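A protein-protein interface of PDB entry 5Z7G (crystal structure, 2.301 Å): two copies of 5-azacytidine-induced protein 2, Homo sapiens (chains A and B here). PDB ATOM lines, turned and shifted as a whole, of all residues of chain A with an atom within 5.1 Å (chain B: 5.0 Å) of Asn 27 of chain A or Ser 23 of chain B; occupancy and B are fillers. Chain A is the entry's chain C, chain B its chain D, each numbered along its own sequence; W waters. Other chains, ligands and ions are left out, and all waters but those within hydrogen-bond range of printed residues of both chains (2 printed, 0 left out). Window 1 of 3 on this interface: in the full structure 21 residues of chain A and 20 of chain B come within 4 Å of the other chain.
The side-chain amide nitrogen of Asn 27 of chain B sits at hydrogen-bond distance from the side-chain carboxylate of Glu 26 of chain A (2.7 Å). The side-chain amide nitrogen (ND2) of Asn 27 of chain A lies within hydrogen-bond range of the backbone carbonyl oxygen (O) of Ser 23 of chain B, at 3.1 Å. ND2 of Asn 27 of chain A lies within hydrogen-bond range of OE2 of Glu 26 of chain B (3.1 Å). The side-chain amide oxygen (OD1) of Asn 27 of chain A lies within hydrogen-bond range of the side-chain amide nitrogen (ND2) of Asn 27 of chain B, 2.8 Å away. The side-chain amino group of Lys 31 of chain A lies within salt-bridge range of the side-chain carboxylate of Glu 26 of chain B (3.0 Å). OG of Ser 23 of chain A sits close to OG of Ser 23 of chain B (2.4 Å).
The side-chain amide oxygen (OD1) of Asn 27 of chain A lies close to the backbone carbonyl oxygen (O) of Ser 23 of chain A.
Arg 19 of chain B touches Leu 20 of chain A (O to CD1, 3.7 Å). CA of Leu 20 of chain A touches CD1 of Leu 20 of chain B, at 3.9 Å. Glu 24 of chain B touches Ser 23 of chain A. N of Glu 24 of chain A touches OG of Ser 23 of chain B, 3.5 Å away. Asn 27 of chain A touches Leu 30 of chain B (O to CD1, 3.6 Å). Asn 27 of chain B touches Leu 30 of chain A. CB of Leu 30 of chain A touches CB of Leu 30 of chain B, 3.99 Å away.
Of chain B, only Ser 23, Glu 26, Asn 27 and Leu 30 come within 4 Å of Asn 27 of chain A. Printed residues of chain A within 4 Å of Glu 24 of chain B: Ser 23 (3.98 Å). Of the printed residues of chain A, Asn 27 of chain B touches Glu 26, Asn 27 and Leu 30. Leu 29 of chain A touches none of the printed residues of chain B. Asp 22 of chain A touches none of the printed residues of chain B.
Hydrophobic or aromatic side chains of chain B within 4 Å of the printed part of chain A: Leu 20 and Leu 30. Hydrophobic or aromatic side chains of chain A that line the printed part of chain B: Leu 20 and Leu 30. Among the printed residues, Asp or Glu carboxylates within 4 Å of a Lys or Arg side-chain nitrogen of the other chain: Lys 31 of chain A with Glu 26 of chain B.
Leu 20 of chain A touches its own counterpart, Leu 20 of chain B. Ser 23 of chain A touches its own counterpart, Ser 23 of chain B. Asn 27 of chain A touches Ser 23 of chain B, but with the chains exchanged Ser 23 of chain A does not touch Asn 27 of chain B (4.3 Å). Asn 27 of chain A touches Leu 30 of chain B, and with the chains exchanged Leu 30 of chain A touches Asn 27 of chain B. 8 positions are printed for both chains.
Water W2 bridges the side-chain carboxylate (OE1) of Glu 24 of chain A (2.8 Å) and the guanidinium group (NE) of Arg 19 of chain B (3.0 Å). Water W1 bridges the side-chain hydroxyl (OG) of Ser 23 of chain A (3.0 Å) and the side-chain amide oxygen (OD1) of Asn 27 of chain B (3.5 Å).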
ATOM      1  N   LEU A  20     -27.176  -9.943 -18.298  1.00  0.00           N
ATOM      2  CA  LEU A  20     -26.928 -10.706 -17.077  1.00  0.00           C
ATOM      3  C   LEU A  20     -28.204 -11.380 -16.584  1.00  0.00           C
ATOM      4  O   LEU A  20     -28.183 -12.559 -16.201  1.00  0.00           O
ATOM      5  CB  LEU A  20     -26.354  -9.811 -15.986  1.00  0.00           C
ATOM      6  CG  LEU A  20     -26.296 -10.456 -14.595  1.00  0.00           C
ATOM      7  CD1 LEU A  20     -25.343 -11.664 -14.585  1.00  0.00           C
ATOM      8  CD2 LEU A  20     -25.891  -9.471 -13.529  1.00  0.00           C
ATOM      9  N   ASP A  22     -30.858 -12.326 -18.243  1.00  0.00           N
ATOM     10  CA  ASP A  22     -31.237 -13.433 -19.114  1.00  0.00           C
ATOM     11  C   ASP A  22     -30.308 -14.617 -18.937  1.00  0.00           C
ATOM     12  O   ASP A  22     -30.749 -15.772 -18.988  1.00  0.00           O
ATOM     13  CB  ASP A  22     -31.230 -12.992 -20.579  1.00  0.00           C
ATOM     14  CG  ASP A  22     -32.278 -11.938 -20.862  1.00  0.00           C
ATOM     15  OD1 ASP A  22     -33.179 -11.769 -20.011  1.00  0.00           O
ATOM     16  OD2 ASP A  22     -32.196 -11.275 -21.916  1.00  0.00           O
ATOM     17  N   SER A  23     -29.018 -14.356 -18.751  1.00  0.00           N
ATOM     18  CA  SER A  23     -28.081 -15.463 -18.644  1.00  0.00           C
ATOM     19  C   SER A  23     -28.303 -16.228 -17.344  1.00  0.00           C
ATOM     20  O   SER A  23     -28.343 -17.461 -17.344  1.00  0.00           O
ATOM     21  CB  SER A  23     -26.654 -14.930 -18.761  1.00  0.00           C
ATOM     22  OG  SER A  23     -25.713 -15.888 -18.356  1.00  0.00           O
ATOM     23  N   GLU A  24     -28.501 -15.509 -16.236  1.00  0.00           N
ATOM     24  CA  GLU A  24     -28.821 -16.154 -14.965  1.00  0.00           C
ATOM     25  C   GLU A  24     -30.169 -16.863 -15.023  1.00  0.00           C
ATOM     26  O   GLU A  24     -30.349 -17.923 -14.412  1.00  0.00           O
ATOM     27  CB  GLU A  24     -28.839 -15.122 -13.838  1.00  0.00           C
ATOM     28  CG  GLU A  24     -27.586 -14.332 -13.707  1.00  0.00           C
ATOM     29  CD  GLU A  24     -26.725 -14.839 -12.608  1.00  0.00           C
ATOM     30  OE1 GLU A  24     -26.470 -14.045 -11.670  1.00  0.00           O
ATOM     31  OE2 GLU A  24     -26.300 -16.019 -12.688  1.00  0.00           O
ATOM     32  N   LYS A  25     -31.142 -16.276 -15.716  1.00  0.00           N
ATOM     33  CA  LYS A  25     -32.426 -16.949 -15.866  1.00  0.00           C
ATOM     34  C   LYS A  25     -32.224 -18.292 -16.554  1.00  0.00           C
ATOM     35  O   LYS A  25     -32.573 -19.347 -16.017  1.00  0.00           O
ATOM     36  CB  LYS A  25     -33.396 -16.068 -16.658  1.00  0.00           C
ATOM     37  CG  LYS A  25     -34.714 -16.757 -17.039  1.00  0.00           C
ATOM     38  CD  LYS A  25     -35.495 -17.136 -15.794  1.00  0.00           C
ATOM     39  CE  LYS A  25     -36.772 -17.901 -16.138  1.00  0.00           C
ATOM     40  NZ  LYS A  25     -37.364 -18.523 -14.908  1.00  0.00           N
ATOM     41  N   GLU A  26     -31.617 -18.267 -17.733  1.00  0.00           N
ATOM     42  CA  GLU A  26     -31.337 -19.510 -18.435  1.00  0.00           C
ATOM     43  C   GLU A  26     -30.540 -20.479 -17.555  1.00  0.00           C
ATOM     44  O   GLU A  26     -30.869 -21.669 -17.474  1.00  0.00           O
ATOM     45  CB  GLU A  26     -30.617 -19.195 -19.752  1.00  0.00           C
ATOM     46  CG  GLU A  26     -30.380 -20.416 -20.648  1.00  0.00           C
ATOM     47  CD  GLU A  26     -29.692 -20.072 -21.958  1.00  0.00           C
ATOM     48  OE1 GLU A  26     -28.461 -20.258 -22.074  1.00  0.00           O
ATOM     49  OE2 GLU A  26     -30.387 -19.617 -22.881  1.00  0.00           O
ATOM     50  N   ASN A  27     -29.532 -19.981 -16.833  1.00  0.00           N
ATOM     51  CA  ASN A  27     -28.731 -20.876 -15.999  1.00  0.00           C
ATOM     52  C   ASN A  27     -29.587 -21.648 -14.999  1.00  0.00           C
ATOM     53  O   ASN A  27     -29.386 -22.853 -14.809  1.00  0.00           O
ATOM     54  CB  ASN A  27     -27.630 -20.096 -15.281  1.00  0.00           C
ATOM     55  CG  ASN A  27     -26.500 -19.739 -16.220  1.00  0.00           C
ATOM     56  OD1 ASN A  27     -26.496 -20.159 -17.374  1.00  0.00           O
ATOM     57  ND2 ASN A  27     -25.550 -18.962 -15.748  1.00  0.00           N
ATOM     58  N   SER A  28     -30.551 -20.982 -14.353  1.00  0.00           N
ATOM     59  CA  SER A  28     -31.394 -21.688 -13.389  1.00  0.00           C
ATOM     60  C   SER A  28     -32.249 -22.742 -14.084  1.00  0.00           C
ATOM     61  O   SER A  28     -32.502 -23.820 -13.532  1.00  0.00           O
ATOM     62  CB  SER A  28     -32.279 -20.695 -12.627  1.00  0.00           C
ATOM     63  OG  SER A  28     -33.382 -20.283 -13.425  1.00  0.00           O
ATOM     64  N   LEU A  29     -32.701 -22.461 -15.302  1.00  0.00           N
ATOM     65  CA  LEU A  29     -33.466 -23.470 -16.027  1.00  0.00           C
ATOM     66  C   LEU A  29     -32.567 -24.614 -16.485  1.00  0.00           C
ATOM     67  O   LEU A  29     -32.974 -25.781 -16.464  1.00  0.00           O
ATOM     68  CB  LEU A  29     -34.185 -22.839 -17.216  1.00  0.00           C
ATOM     69  CG  LEU A  29     -35.066 -21.620 -16.937  1.00  0.00           C
ATOM     70  CD1 LEU A  29     -35.886 -21.292 -18.187  1.00  0.00           C
ATOM     71  CD2 LEU A  29     -35.954 -21.863 -15.699  1.00  0.00           C
ATOM     72  N   LEU A  30     -31.338 -24.302 -16.888  1.00  0.00           N
ATOM     73  CA  LEU A  30     -30.404 -25.362 -17.260  1.00  0.00           C
ATOM     74  C   LEU A  30     -30.163 -26.313 -16.093  1.00  0.00           C
ATOM     75  O   LEU A  30     -30.065 -27.531 -16.288  1.00  0.00           O
ATOM     76  CB  LEU A  30     -29.082 -24.757 -17.757  1.00  0.00           C
ATOM     77  CG  LEU A  30     -29.142 -23.930 -19.056  1.00  0.00           C
ATOM     78  CD1 LEU A  30     -27.822 -23.205 -19.329  1.00  0.00           C
ATOM     79  CD2 LEU A  30     -29.554 -24.774 -20.264  1.00  0.00           C
ATOM     80  N   LYS A  31     -30.093 -25.773 -14.867  1.00  0.00           N
ATOM     81  CA  LYS A  31     -29.924 -26.613 -13.682  1.00  0.00           C
ATOM     82  C   LYS A  31     -31.136 -27.500 -13.458  1.00  0.00           C
ATOM     83  O   LYS A  31     -30.996 -28.657 -13.043  1.00  0.00           O
ATOM     84  CB  LYS A  31     -29.682 -25.749 -12.443  1.00  0.00           C
ATOM     85  CG  LYS A  31     -28.300 -25.127 -12.403  1.00  0.00           C
ATOM     86  CD  LYS A  31     -28.184 -24.008 -11.376  1.00  0.00           C
ATOM     87  CE  LYS A  31     -26.730 -23.521 -11.321  1.00  0.00           C
ATOM     88  NZ  LYS A  31     -26.551 -22.063 -11.002  1.00  0.00           N
ATOM     89  N   ARG B  19     -19.959  -9.996 -13.299  1.00  0.00           N
ATOM     90  CA  ARG B  19     -20.943 -11.029 -13.037  1.00  0.00           C
ATOM     91  C   ARG B  19     -21.486 -11.621 -14.323  1.00  0.00           C
ATOM     92  O   ARG B  19     -21.788 -12.815 -14.367  1.00  0.00           O
ATOM     93  CB  ARG B  19     -22.053 -10.465 -12.168  1.00  0.00           C
ATOM     94  CG  ARG B  19     -21.515 -10.191 -10.764  1.00  0.00           C
ATOM     95  CD  ARG B  19     -22.346  -9.163 -10.036  1.00  0.00           C
ATOM     96  NE  ARG B  19     -23.709  -9.626  -9.804  1.00  0.00           N
ATOM     97  CZ  ARG B  19     -24.574  -8.996  -9.011  1.00  0.00           C
ATOM     98  NH1 ARG B  19     -24.210  -7.869  -8.386  1.00  0.00           N
ATOM     99  NH2 ARG B  19     -25.803  -9.482  -8.856  1.00  0.00           N
ATOM    100  N   LEU B  20     -21.584 -10.825 -15.387  1.00  0.00           N
ATOM    101  CA  LEU B  20     -21.961 -11.387 -16.678  1.00  0.00           C
ATOM    102  C   LEU B  20     -20.937 -12.423 -17.134  1.00  0.00           C
ATOM    103  O   LEU B  20     -21.300 -13.523 -17.573  1.00  0.00           O
ATOM    104  CB  LEU B  20     -22.107 -10.281 -17.725  1.00  0.00           C
ATOM    105  CG  LEU B  20     -22.436 -10.750 -19.146  1.00  0.00           C
ATOM    106  CD1 LEU B  20     -23.735 -11.565 -19.116  1.00  0.00           C
ATOM    107  CD2 LEU B  20     -22.578  -9.565 -20.082  1.00  0.00           C
ATOM    108  N   LYS B  21     -19.643 -12.100 -17.021  1.00  0.00           N
ATOM    109  CA  LYS B  21     -18.627 -13.059 -17.451  1.00  0.00           C
ATOM    110  C   LYS B  21     -18.698 -14.350 -16.635  1.00  0.00           C
ATOM    111  O   LYS B  21     -18.646 -15.446 -17.206  1.00  0.00           O
ATOM    112  CB  LYS B  21     -17.234 -12.436 -17.376  1.00  0.00           C
ATOM    113  CG  LYS B  21     -17.156 -11.043 -18.010  1.00  0.00           C
ATOM    114  CD  LYS B  21     -15.763 -10.777 -18.627  1.00  0.00           C
ATOM    115  CE  LYS B  21     -15.398  -9.299 -18.595  1.00  0.00           C
ATOM    116  NZ  LYS B  21     -14.925  -8.881 -17.240  1.00  0.00           N
ATOM    117  N   ASP B  22     -18.856 -14.250 -15.308  1.00  0.00           N
ATOM    118  CA  ASP B  22     -19.085 -15.460 -14.515  1.00  0.00           C
ATOM    119  C   ASP B  22     -20.320 -16.222 -14.985  1.00  0.00           C
ATOM    120  O   ASP B  22     -20.295 -17.455 -15.094  1.00  0.00           O
ATOM    121  CB  ASP B  22     -19.231 -15.108 -13.038  1.00  0.00           C
ATOM    122  CG  ASP B  22     -17.948 -14.571 -12.434  1.00  0.00           C
ATOM    123  OD1 ASP B  22     -16.856 -14.896 -12.948  1.00  0.00           O
ATOM    124  OD2 ASP B  22     -18.039 -13.831 -11.429  1.00  0.00           O
ATOM    125  N   SER B  23     -21.416 -15.514 -15.255  1.00  0.00           N
ATOM    126  CA  SER B  23     -22.645 -16.171 -15.705  1.00  0.00           C
ATOM    127  C   SER B  23     -22.475 -16.874 -17.044  1.00  0.00           C
ATOM    128  O   SER B  23     -23.003 -17.969 -17.249  1.00  0.00           O
ATOM    129  CB  SER B  23     -23.781 -15.166 -15.819  1.00  0.00           C
ATOM    130  OG  SER B  23     -25.005 -15.849 -16.068  1.00  0.00           O
ATOM    131  N   GLU B  24     -21.767 -16.246 -17.972  1.00  0.00           N
ATOM    132  CA  GLU B  24     -21.583 -16.869 -19.275  1.00  0.00           C
ATOM    133  C   GLU B  24     -20.698 -18.104 -19.170  1.00  0.00           C
ATOM    134  O   GLU B  24     -20.935 -19.098 -19.858  1.00  0.00           O
ATOM    135  CB  GLU B  24     -21.003 -15.848 -20.247  1.00  0.00           C
ATOM    136  CG  GLU B  24     -22.011 -14.776 -20.606  1.00  0.00           C
ATOM    137  CD  GLU B  24     -21.497 -13.786 -21.634  1.00  0.00           C
ATOM    138  OE1 GLU B  24     -20.274 -13.539 -21.688  1.00  0.00           O
ATOM    139  OE2 GLU B  24     -22.339 -13.270 -22.408  1.00  0.00           O
ATOM    140  N   LYS B  25     -19.694 -18.074 -18.297  1.00  0.00           N
ATOM    141  CA  LYS B  25     -18.876 -19.269 -18.119  1.00  0.00           C
ATOM    142  C   LYS B  25     -19.691 -20.412 -17.523  1.00  0.00           C
ATOM    143  O   LYS B  25     -19.556 -21.562 -17.951  1.00  0.00           O
ATOM    144  CB  LYS B  25     -17.656 -18.948 -17.254  1.00  0.00           C
ATOM    145  CG  LYS B  25     -16.789 -20.152 -16.976  1.00  0.00           C
ATOM    146  CD  LYS B  25     -15.407 -19.731 -16.471  1.00  0.00           C
ATOM    147  CE  LYS B  25     -15.269 -19.889 -14.957  1.00  0.00           C
ATOM    148  NZ  LYS B  25     -14.133 -20.784 -14.570  1.00  0.00           N
ATOM    149  N   GLU B  26     -20.538 -20.129 -16.523  1.00  0.00           N
ATOM    150  CA  GLU B  26     -21.404 -21.171 -15.984  1.00  0.00           C
ATOM    151  C   GLU B  26     -22.346 -21.698 -17.064  1.00  0.00           C
ATOM    152  O   GLU B  26     -22.539 -22.911 -17.202  1.00  0.00           O
ATOM    153  CB  GLU B  26     -22.189 -20.633 -14.783  1.00  0.00           C
ATOM    154  CG  GLU B  26     -22.530 -21.698 -13.736  1.00  0.00           C
ATOM    155  CD  GLU B  26     -23.774 -21.361 -12.905  1.00  0.00           C
ATOM    156  OE1 GLU B  26     -23.721 -21.479 -11.666  1.00  0.00           O
ATOM    157  OE2 GLU B  26     -24.815 -20.986 -13.483  1.00  0.00           O
ATOM    158  N   ASN B  27     -22.924 -20.786 -17.852  1.00  0.00           N
ATOM    159  CA  ASN B  27     -23.786 -21.161 -18.961  1.00  0.00           C
ATOM    160  C   ASN B  27     -23.108 -22.196 -19.855  1.00  0.00           C
ATOM    161  O   ASN B  27     -23.710 -23.215 -20.214  1.00  0.00           O
ATOM    162  CB  ASN B  27     -24.155 -19.904 -19.753  1.00  0.00           C
ATOM    163  CG  ASN B  27     -25.298 -20.134 -20.722  1.00  0.00           C
ATOM    164  OD1 ASN B  27     -25.088 -20.287 -21.925  1.00  0.00           O
ATOM    165  ND2 ASN B  27     -26.521 -20.165 -20.199  1.00  0.00           N
ATOM    166  N   LEU B  30     -22.844 -25.595 -17.843  1.00  0.00           N
ATOM    167  CA  LEU B  30     -24.123 -26.289 -17.698  1.00  0.00           C
ATOM    168  C   LEU B  30     -24.577 -26.869 -19.026  1.00  0.00           C
ATOM    169  O   LEU B  30     -25.129 -27.976 -19.071  1.00  0.00           O
ATOM    170  CB  LEU B  30     -25.188 -25.352 -17.137  1.00  0.00           C
ATOM    171  CG  LEU B  30     -24.882 -24.702 -15.780  1.00  0.00           C
ATOM    172  CD1 LEU B  30     -25.891 -23.586 -15.494  1.00  0.00           C
ATOM    173  CD2 LEU B  30     -24.874 -25.723 -14.654  1.00  0.00           C
HETATM  174  O   HOH W   1     -25.239 -16.935 -21.073  1.00  0.00           O
HETATM  175  O   HOH W   2     -24.801 -12.444 -10.158  1.00  0.00           O
